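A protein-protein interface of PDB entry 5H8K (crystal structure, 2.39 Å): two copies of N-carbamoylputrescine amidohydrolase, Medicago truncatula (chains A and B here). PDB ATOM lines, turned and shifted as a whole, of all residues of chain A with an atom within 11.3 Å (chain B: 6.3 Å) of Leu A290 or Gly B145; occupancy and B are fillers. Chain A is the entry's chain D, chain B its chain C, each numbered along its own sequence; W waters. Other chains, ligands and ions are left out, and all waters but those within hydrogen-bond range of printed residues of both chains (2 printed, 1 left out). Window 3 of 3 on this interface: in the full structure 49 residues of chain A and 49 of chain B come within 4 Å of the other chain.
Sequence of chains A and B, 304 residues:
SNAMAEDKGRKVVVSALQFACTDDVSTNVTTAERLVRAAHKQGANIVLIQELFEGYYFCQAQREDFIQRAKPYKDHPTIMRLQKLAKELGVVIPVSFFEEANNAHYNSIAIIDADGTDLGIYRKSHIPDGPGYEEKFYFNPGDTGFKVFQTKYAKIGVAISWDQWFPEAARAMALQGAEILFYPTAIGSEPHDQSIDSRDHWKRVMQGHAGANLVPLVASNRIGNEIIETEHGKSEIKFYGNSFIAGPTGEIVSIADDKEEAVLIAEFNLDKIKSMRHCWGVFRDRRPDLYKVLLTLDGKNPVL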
ATOM      1  N   ASP A 285     -21.703   4.543 -21.618  1.00  0.00           N
ATOM      2  CA  ASP A 285     -20.301   4.746 -21.243  1.00  0.00           C
ATOM      3  C   ASP A 285     -20.058   5.866 -20.186  1.00  0.00           C
ATOM      4  O   ASP A 285     -18.928   6.047 -19.741  1.00  0.00           O
ATOM      5  CB  ASP A 285     -19.459   5.008 -22.488  1.00  0.00           C
ATOM      6  CG  ASP A 285     -19.476   3.859 -23.475  1.00  0.00           C
ATOM      7  OD1 ASP A 285     -19.829   2.713 -23.091  1.00  0.00           O
ATOM      8  OD2 ASP A 285     -19.131   4.090 -24.642  1.00  0.00           O
ATOM      9  N   ARG A 286     -21.117   6.564 -19.779  1.00  0.00           N
ATOM     10  CA  ARG A 286     -20.995   7.626 -18.791  1.00  0.00           C
ATOM     11  C   ARG A 286     -20.496   7.090 -17.461  1.00  0.00           C
ATOM     12  O   ARG A 286     -20.645   5.869 -17.124  1.00  0.00           O
ATOM     13  CB  ARG A 286     -22.331   8.323 -18.591  1.00  0.00           C
ATOM     14  CG  ARG A 286     -22.724   9.219 -19.723  1.00  0.00           C
ATOM     15  CD  ARG A 286     -24.091   9.853 -19.599  1.00  0.00           C
ATOM     16  NE  ARG A 286     -24.055  10.856 -18.579  1.00  0.00           N
ATOM     17  CZ  ARG A 286     -24.508  10.682 -17.352  1.00  0.00           C
ATOM     18  NH1 ARG A 286     -25.090   9.542 -17.017  1.00  0.00           N
ATOM     19  NH2 ARG A 286     -24.411  11.660 -16.463  1.00  0.00           N
ATOM     20  N   ARG A 287     -19.882   8.016 -16.730  1.00  0.00           N
ATOM     21  CA  ARG A 287     -19.223   7.728 -15.448  1.00  0.00           C
ATOM     22  C   ARG A 287     -19.700   8.676 -14.335  1.00  0.00           C
ATOM     23  O   ARG A 287     -18.934   9.480 -13.812  1.00  0.00           O
ATOM     24  CB  ARG A 287     -17.710   7.887 -15.578  1.00  0.00           C
ATOM     25  CG  ARG A 287     -17.034   7.029 -16.612  1.00  0.00           C
ATOM     26  CD  ARG A 287     -16.887   5.604 -16.171  1.00  0.00           C
ATOM     27  NE  ARG A 287     -16.394   5.486 -14.811  1.00  0.00           N
ATOM     28  CZ  ARG A 287     -15.112   5.350 -14.484  1.00  0.00           C
ATOM     29  NH1 ARG A 287     -14.177   5.358 -15.433  1.00  0.00           N
ATOM     30  NH2 ARG A 287     -14.752   5.247 -13.177  1.00  0.00           N
ATOM     31  N   PRO A 288     -20.966   8.557 -13.932  1.00  0.00           N
ATOM     32  CA  PRO A 288     -21.458   9.326 -12.809  1.00  0.00           C
ATOM     33  C   PRO A 288     -20.603   9.211 -11.558  1.00  0.00           C
ATOM     34  O   PRO A 288     -20.572  10.158 -10.795  1.00  0.00           O
ATOM     35  CB  PRO A 288     -22.861   8.744 -12.563  1.00  0.00           C
ATOM     36  CG  PRO A 288     -22.933   7.453 -13.324  1.00  0.00           C
ATOM     37  CD  PRO A 288     -21.990   7.644 -14.466  1.00  0.00           C
ATOM     38  N   ASP A 289     -19.880   8.113 -11.374  1.00  0.00           N
ATOM     39  CA  ASP A 289     -18.982   7.968 -10.184  1.00  0.00           C
ATOM     40  C   ASP A 289     -17.874   9.010 -10.147  1.00  0.00           C
ATOM     41  O   ASP A 289     -17.299   9.252  -9.087  1.00  0.00           O
ATOM     42  CB  ASP A 289     -18.377   6.531 -10.043  1.00  0.00           C
ATOM     43  CG  ASP A 289     -17.663   5.991 -11.347  1.00  0.00           C
ATOM     44  OD1 ASP A 289     -18.054   6.347 -12.472  1.00  0.00           O
ATOM     45  OD2 ASP A 289     -16.726   5.197 -11.222  1.00  0.00           O
ATOM     46  N   LEU A 290     -17.581   9.616 -11.315  1.00  0.00           N
ATOM     47  CA  LEU A 290     -16.497  10.558 -11.474  1.00  0.00           C
ATOM     48  C   LEU A 290     -17.042  11.955 -11.696  1.00  0.00           C
ATOM     49  O   LEU A 290     -16.253  12.896 -11.886  1.00  0.00           O
ATOM     50  CB  LEU A 290     -15.629  10.204 -12.716  1.00  0.00           C
ATOM     51  CG  LEU A 290     -14.888   8.867 -12.718  1.00  0.00           C
ATOM     52  CD1 LEU A 290     -14.075   8.787 -14.009  1.00  0.00           C
ATOM     53  CD2 LEU A 290     -14.003   8.680 -11.477  1.00  0.00           C
ATOM     54  N   TYR A 291     -18.358  12.098 -11.682  1.00  0.00           N
ATOM     55  CA  TYR A 291     -18.987  13.422 -11.905  1.00  0.00           C
ATOM     56  C   TYR A 291     -19.345  14.273 -10.640  1.00  0.00           C
ATOM     57  O   TYR A 291     -19.921  15.362 -10.767  1.00  0.00           O
ATOM     58  CB  TYR A 291     -20.237  13.298 -12.813  1.00  0.00           C
ATOM     59  CG  TYR A 291     -20.011  12.630 -14.147  1.00  0.00           C
ATOM     60  CD1 TYR A 291     -18.790  12.629 -14.779  1.00  0.00           C
ATOM     61  CD2 TYR A 291     -21.055  12.037 -14.812  1.00  0.00           C
ATOM     62  CE1 TYR A 291     -18.625  12.048 -16.033  1.00  0.00           C
ATOM     63  CE2 TYR A 291     -20.889  11.464 -16.095  1.00  0.00           C
ATOM     64  CZ  TYR A 291     -19.668  11.459 -16.679  1.00  0.00           C
ATOM     65  OH  TYR A 291     -19.557  10.827 -17.916  1.00  0.00           O
ATOM     66  N   LYS A 292     -18.943  13.852  -9.457  1.00  0.00           N
ATOM     67  CA  LYS A 292     -19.358  14.559  -8.253  1.00  0.00           C
ATOM     68  C   LYS A 292     -18.931  16.038  -8.277  1.00  0.00           C
ATOM     69  O   LYS A 292     -19.598  16.881  -7.704  1.00  0.00           O
ATOM     70  CB  LYS A 292     -18.786  13.891  -7.040  1.00  0.00           C
ATOM     71  CG  LYS A 292     -19.609  12.709  -6.589  1.00  0.00           C
ATOM     72  CD  LYS A 292     -18.944  12.009  -5.442  1.00  0.00           C
ATOM     73  CE  LYS A 292     -19.910  11.025  -4.785  1.00  0.00           C
ATOM     74  NZ  LYS A 292     -19.658   9.623  -5.260  1.00  0.00           N
ATOM     75  N   VAL A 293     -17.843  16.339  -8.992  1.00  0.00           N
ATOM     76  CA  VAL A 293     -17.325  17.682  -9.049  1.00  0.00           C
ATOM     77  C   VAL A 293     -18.297  18.617  -9.741  1.00  0.00           C
ATOM     78  O   VAL A 293     -18.215  19.819  -9.525  1.00  0.00           O
ATOM     79  CB  VAL A 293     -15.960  17.758  -9.756  1.00  0.00           C
ATOM     80  CG1 VAL A 293     -16.122  17.548 -11.256  1.00  0.00           C
ATOM     81  CG2 VAL A 293     -15.318  19.080  -9.472  1.00  0.00           C
ATOM     82  N   LEU A 294     -19.237  18.081 -10.505  1.00  0.00           N
ATOM     83  CA  LEU A 294     -20.243  18.963 -11.090  1.00  0.00           C
ATOM     84  C   LEU A 294     -21.195  19.518 -10.059  1.00  0.00           C
ATOM     85  O   LEU A 294     -22.041  20.340 -10.396  1.00  0.00           O
ATOM     86  CB  LEU A 294     -21.078  18.268 -12.172  1.00  0.00           C
ATOM     87  CG  LEU A 294     -20.287  17.519 -13.258  1.00  0.00           C
ATOM     88  CD1 LEU A 294     -21.213  16.945 -14.310  1.00  0.00           C
ATOM     89  CD2 LEU A 294     -19.268  18.440 -13.908  1.00  0.00           C
ATOM     90  N   LEU A 295     -21.120  19.022  -8.815  1.00  0.00           N
ATOM     91  CA  LEU A 295     -22.072  19.485  -7.815  1.00  0.00           C
ATOM     92  C   LEU A 295     -21.362  20.564  -7.040  1.00  0.00           C
ATOM     93  O   LEU A 295     -21.773  20.932  -5.954  1.00  0.00           O
ATOM     94  CB  LEU A 295     -22.528  18.347  -6.886  1.00  0.00           C
ATOM     95  CG  LEU A 295     -23.295  17.192  -7.548  1.00  0.00           C
ATOM     96  CD1 LEU A 295     -23.973  16.277  -6.546  1.00  0.00           C
ATOM     97  CD2 LEU A 295     -24.340  17.625  -8.525  1.00  0.00           C
ATOM     98  N   THR A 296     -20.245  21.024  -7.580  1.00  0.00           N
ATOM     99  CA  THR A 296     -19.549  22.180  -7.003  1.00  0.00           C
ATOM    100  C   THR A 296     -19.760  23.385  -7.908  1.00  0.00           C
ATOM    101  O   THR A 296     -20.157  23.232  -9.069  1.00  0.00           O
ATOM    102  CB  THR A 296     -18.013  21.943  -6.841  1.00  0.00           C
ATOM    103  OG1 THR A 296     -17.323  21.989  -8.126  1.00  0.00           O
ATOM    104  CG2 THR A 296     -17.738  20.602  -6.148  1.00  0.00           C
ATOM    105  N   GLY A 299     -15.135  24.074  -8.010  1.00  0.00           N
ATOM    106  CA  GLY A 299     -14.259  22.938  -8.294  1.00  0.00           C
ATOM    107  C   GLY A 299     -13.776  22.082  -7.125  1.00  0.00           C
ATOM    108  O   GLY A 299     -13.059  21.169  -7.338  1.00  0.00           O
ATOM    109  N   ILE B 121      -0.380  11.493 -14.123  1.00  0.00           N
ATOM    110  CA  ILE B 121      -1.159  10.872 -15.163  1.00  0.00           C
ATOM    111  C   ILE B 121      -2.646  11.077 -15.020  1.00  0.00           C
ATOM    112  O   ILE B 121      -3.180  11.380 -13.949  1.00  0.00           O
ATOM    113  CB  ILE B 121      -0.942   9.347 -15.236  1.00  0.00           C
ATOM    114  CG1 ILE B 121      -1.167   8.718 -13.881  1.00  0.00           C
ATOM    115  CG2 ILE B 121       0.469   9.025 -15.648  1.00  0.00           C
ATOM    116  CD1 ILE B 121      -1.266   7.238 -14.067  1.00  0.00           C
ATOM    117  N   TYR B 122      -3.289  10.928 -16.164  1.00  0.00           N
ATOM    118  CA  TYR B 122      -4.731  10.888 -16.246  1.00  0.00           C
ATOM    119  C   TYR B 122      -5.020   9.530 -16.887  1.00  0.00           C
ATOM    120  O   TYR B 122      -4.283   9.120 -17.833  1.00  0.00           O
ATOM    121  CB  TYR B 122      -5.295  12.048 -17.103  1.00  0.00           C
ATOM    122  CG  TYR B 122      -6.708  11.776 -17.502  1.00  0.00           C
ATOM    123  CD1 TYR B 122      -7.733  11.861 -16.581  1.00  0.00           C
ATOM    124  CD2 TYR B 122      -7.034  11.383 -18.811  1.00  0.00           C
ATOM    125  CE1 TYR B 122      -9.062  11.568 -16.919  1.00  0.00           C
ATOM    126  CE2 TYR B 122      -8.368  11.104 -19.169  1.00  0.00           C
ATOM    127  CZ  TYR B 122      -9.387  11.213 -18.215  1.00  0.00           C
ATOM    128  OH  TYR B 122     -10.694  10.889 -18.534  1.00  0.00           O
ATOM    129  N   ARG B 123      -6.047   8.847 -16.370  1.00  0.00           N
ATOM    130  CA  ARG B 123      -6.467   7.570 -16.904  1.00  0.00           C
ATOM    131  C   ARG B 123      -7.828   7.708 -17.585  1.00  0.00           C
ATOM    132  O   ARG B 123      -8.775   8.199 -16.967  1.00  0.00           O
ATOM    133  CB  ARG B 123      -6.519   6.501 -15.795  1.00  0.00           C
ATOM    134  CG  ARG B 123      -5.135   6.041 -15.351  1.00  0.00           C
ATOM    135  CD  ARG B 123      -5.170   5.181 -14.046  1.00  0.00           C
ATOM    136  NE  ARG B 123      -3.906   4.490 -13.769  1.00  0.00           N
ATOM    137  CZ  ARG B 123      -3.633   3.844 -12.624  1.00  0.00           C
ATOM    138  NH1 ARG B 123      -4.517   3.838 -11.638  1.00  0.00           N
ATOM    139  NH2 ARG B 123      -2.464   3.207 -12.472  1.00  0.00           N
ATOM    140  N   SER B 125     -11.392   7.819 -18.741  1.00  0.00           N
ATOM    141  CA  SER B 125     -12.561   7.459 -17.978  1.00  0.00           C
ATOM    142  C   SER B 125     -13.665   6.781 -18.782  1.00  0.00           C
ATOM    143  O   SER B 125     -14.327   5.837 -18.302  1.00  0.00           O
ATOM    144  CB  SER B 125     -13.147   8.710 -17.359  1.00  0.00           C
ATOM    145  OG  SER B 125     -12.195   9.399 -16.593  1.00  0.00           O
ATOM    146  N   HIS B 126     -13.921   7.317 -19.969  1.00  0.00           N
ATOM    147  CA  HIS B 126     -14.957   6.775 -20.838  1.00  0.00           C
ATOM    148  C   HIS B 126     -14.340   5.878 -21.911  1.00  0.00           C
ATOM    149  O   HIS B 126     -13.483   6.324 -22.669  1.00  0.00           O
ATOM    150  CB  HIS B 126     -15.739   7.920 -21.525  1.00  0.00           C
ATOM    151  CG  HIS B 126     -16.209   8.992 -20.586  1.00  0.00           C
ATOM    152  ND1 HIS B 126     -15.436  10.077 -20.270  1.00  0.00           N
ATOM    153  CD2 HIS B 126     -17.378   9.156 -19.921  1.00  0.00           C
ATOM    154  CE1 HIS B 126     -16.111  10.875 -19.459  1.00  0.00           C
ATOM    155  NE2 HIS B 126     -17.296  10.349 -19.241  1.00  0.00           N
ATOM    156  N   GLY B 142     -10.963   4.254 -16.315  1.00  0.00           N
ATOM    157  CA  GLY B 142     -10.132   5.076 -15.494  1.00  0.00           C
ATOM    158  C   GLY B 142     -10.642   5.396 -14.099  1.00  0.00           C
ATOM    159  O   GLY B 142     -11.870   5.525 -13.837  1.00  0.00           O
ATOM    160  N   ASP B 143      -9.657   5.499 -13.203  1.00  0.00           N
ATOM    161  CA  ASP B 143      -9.894   5.688 -11.838  1.00  0.00           C
ATOM    162  C   ASP B 143      -9.221   6.937 -11.255  1.00  0.00           C
ATOM    163  O   ASP B 143      -9.338   7.175 -10.067  1.00  0.00           O
ATOM    164  CB  ASP B 143      -9.582   4.394 -11.040  1.00  0.00           C
ATOM    165  CG  ASP B 143      -8.147   3.824 -11.239  1.00  0.00           C
ATOM    166  OD1 ASP B 143      -7.237   4.552 -11.655  1.00  0.00           O
ATOM    167  OD2 ASP B 143      -7.936   2.626 -10.976  1.00  0.00           O
ATOM    168  N   THR B 144      -8.623   7.794 -12.058  1.00  0.00           N
ATOM    169  CA  THR B 144      -8.055   9.035 -11.524  1.00  0.00           C
ATOM    170  C   THR B 144      -9.069  10.117 -11.370  1.00  0.00           C
ATOM    171  O   THR B 144      -8.890  11.038 -10.618  1.00  0.00           O
ATOM    172  CB  THR B 144      -7.023   9.624 -12.468  1.00  0.00           C
ATOM    173  OG1 THR B 144      -7.625   9.827 -13.806  1.00  0.00           O
ATOM    174  CG2 THR B 144      -5.820   8.695 -12.532  1.00  0.00           C
ATOM    175  N   GLY B 145     -10.165  10.012 -12.079  1.00  0.00           N
ATOM    176  CA  GLY B 145     -11.007  11.176 -12.265  1.00  0.00           C
ATOM    177  C   GLY B 145     -10.378  12.208 -13.191  1.00  0.00           C
ATOM    178  O   GLY B 145      -9.227  12.077 -13.589  1.00  0.00           O
ATOM    179  N   PHE B 146     -11.190  13.204 -13.566  1.00  0.00           N
ATOM    180  CA  PHE B 146     -10.753  14.335 -14.357  1.00  0.00           C
ATOM    181  C   PHE B 146      -9.853  15.212 -13.517  1.00  0.00           C
ATOM    182  O   PHE B 146     -10.134  15.505 -12.337  1.00  0.00           O
ATOM    183  CB  PHE B 146     -11.966  15.058 -14.905  1.00  0.00           C
ATOM    184  CG  PHE B 146     -12.930  14.108 -15.541  1.00  0.00           C
ATOM    185  CD1 PHE B 146     -12.569  13.426 -16.707  1.00  0.00           C
ATOM    186  CD2 PHE B 146     -14.118  13.762 -14.904  1.00  0.00           C
ATOM    187  CE1 PHE B 146     -13.382  12.452 -17.253  1.00  0.00           C
ATOM    188  CE2 PHE B 146     -14.955  12.812 -15.440  1.00  0.00           C
ATOM    189  CZ  PHE B 146     -14.595  12.172 -16.629  1.00  0.00           C
ATOM    190  N   LYS B 147      -8.730  15.550 -14.126  1.00  0.00           N
ATOM    191  CA  LYS B 147      -7.607  16.257 -13.515  1.00  0.00           C
ATOM    192  C   LYS B 147      -7.229  17.496 -14.334  1.00  0.00           C
ATOM    193  O   LYS B 147      -7.485  17.543 -15.542  1.00  0.00           O
ATOM    194  CB  LYS B 147      -6.417  15.315 -13.502  1.00  0.00           C
ATOM    195  CG  LYS B 147      -6.572  14.271 -12.401  1.00  0.00           C
ATOM    196  CD  LYS B 147      -5.415  13.299 -12.393  1.00  0.00           C
ATOM    197  CE  LYS B 147      -4.241  13.845 -11.596  1.00  0.00           C
ATOM    198  NZ  LYS B 147      -3.146  12.811 -11.468  1.00  0.00           N
ATOM    199  N   ALA B 172     -15.901  19.327 -15.904  1.00  0.00           N
ATOM    200  CA  ALA B 172     -15.189  18.966 -14.653  1.00  0.00           C
ATOM    201  C   ALA B 172     -13.790  19.554 -14.674  1.00  0.00           C
ATOM    202  O   ALA B 172     -13.247  19.980 -13.628  1.00  0.00           O
ATOM    203  CB  ALA B 172     -15.081  17.447 -14.515  1.00  0.00           C
ATOM    204  N   LEU B 295     -25.675  12.278 -11.645  1.00  0.00           N
ATOM    205  CA  LEU B 295     -25.048  11.154 -10.967  1.00  0.00           C
ATOM    206  C   LEU B 295     -25.822   9.816 -11.092  1.00  0.00           C
ATOM    207  O   LEU B 295     -25.544   8.822 -10.376  1.00  0.00           O
ATOM    208  CB  LEU B 295     -24.885  11.490  -9.472  1.00  0.00           C
ATOM    209  CG  LEU B 295     -24.051  12.763  -9.206  1.00  0.00           C
ATOM    210  CD1 LEU B 295     -23.754  12.950  -7.713  1.00  0.00           C
ATOM    211  CD2 LEU B 295     -22.757  12.754  -9.978  1.00  0.00           C
HETATM  212  O   HOH W   1     -12.852   2.524 -12.385  1.00  0.00           O
HETATM  213  O   HOH W   2     -13.054   4.614 -10.705  1.00  0.00           O
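The side-chain hydroxyl (OH) of Tyr A291 lies within hydrogen-bond range of a ring nitrogen (NE2) of His B126 (2.7 Å). The backbone carbonyl oxygen of Ser B125 sits at hydrogen-bond distance from the guanidinium group of Arg A287 (2.9 Å). The backbone carbonyl oxygen (O) of Gly B142 lies within hydrogen-bond range of the guanidinium group (NH1) of Arg A287 (2.8 Å).
The side-chain hydroxyl (OH) of Tyr A291 lies within hydrogen-bond range of the backbone NH (N) of Arg A287, 3.1 Å away. The side-chain hydroxyl (OH) of Tyr B122 is in hydrogen-bond range of the side-chain hydroxyl (OG) of Ser B125 (2.9 Å). The guanidinium group of Arg A287 is in salt-bridge range of the side-chain carboxylate of Asp A289, at 2.8 Å. O of Val A293 sits at hydrogen-bond distance from OG1 of Thr A296, 2.7 Å away.
Asp A285 touches His B126 (O to CD2, 3.5 Å). CG of Arg A287 touches CD2 of His B126 (3.9 Å). OG of Ser B125 touches CD1 of Leu A290, 3.3 Å away. O of Gly B142 touches CD1 of Leu A290, 3.9 Å away. Leu A290 touches Gly B145 (CD2 to CA, 3.98 Å). O of Leu A290 touches CE2 of Phe B146, 3.8 Å away. CE1 of Tyr A291 touches CE2 of Phe B146, at 3.8 Å. Leu B295 touches Tyr A291 (CD2 to C, 3.8 Å). Val A293 touches Ala B172 (CG1 to CB, 3.4 Å). CD1 of Leu B295 touches CD1 of Leu A295, at 3.5 Å.
Leu A290 touches just these residues of chain B: Ser B125 (3.3 Å), Gly B142 (3.9 Å), Gly B145 (3.98 Å) and Phe B146 (3.8 Å). Gly B145 touches one residue of chain A. No residue of chain A comes within 4 Å of Tyr B122. Ser B125 touches two residues of chain A. Gly B142 touches two residues of chain A. No residue of chain A comes within 4 Å of Lys B147. Printed residues of chain A within 4 Å of Leu B295: Pro A288, Tyr A291 and Leu A295. Printed residues of chain B within 4 Å of Leu A295: Leu B295. Of the printed residues of chain B, Pro A288 touches Leu B295. Of the printed residues of chain B, Val A293 touches Ala B172 (3.4 Å). Printed residues of chain B within 4 Å of Tyr A291: His B126 (2.7 Å), Phe B146 (3.8 Å) and Leu B295 (3.8 Å). Thr A296 touches none of the printed residues of chain B. The nearest residue of chain A that does not touch Gly B145 is Arg A287 (6.7 Å).
Hydrophobic or aromatic side chains of chain B within 4 Å of the printed part of chain A: His B126, Phe B146, Ala B172 and Leu B295. Of the 13 printed residues of chain A, 7 touch a printed residue of chain B. Hydrophobic or aromatic side chains of chain A that line the printed part of chain B: Pro A288, Leu A290, Tyr A291, Val A293 and Leu A295. Among the printed residues, 14 pairs touch across the chains. Among the printed residues, no Asp or Glu carboxylate lies within 4 Å of a Lys or Arg side-chain nitrogen of the other chain.
Leu A295 touches its own counterpart, Leu B295. Of the 14 pairs that touch across the chains among the printed residues, 1 has its exchanged pair printed and touching as well.
Water W2 lies within hydrogen-bond range of the guanidinium group of Arg A287 (3.1 Å) and the backbone carbonyl oxygen of Gly B142 (3.5 Å). Water W1 lies within hydrogen-bond range of the guanidinium group of Arg A287 (3.4 Å) and the backbone carbonyl oxygen of Gly B142 (3.5 Å).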
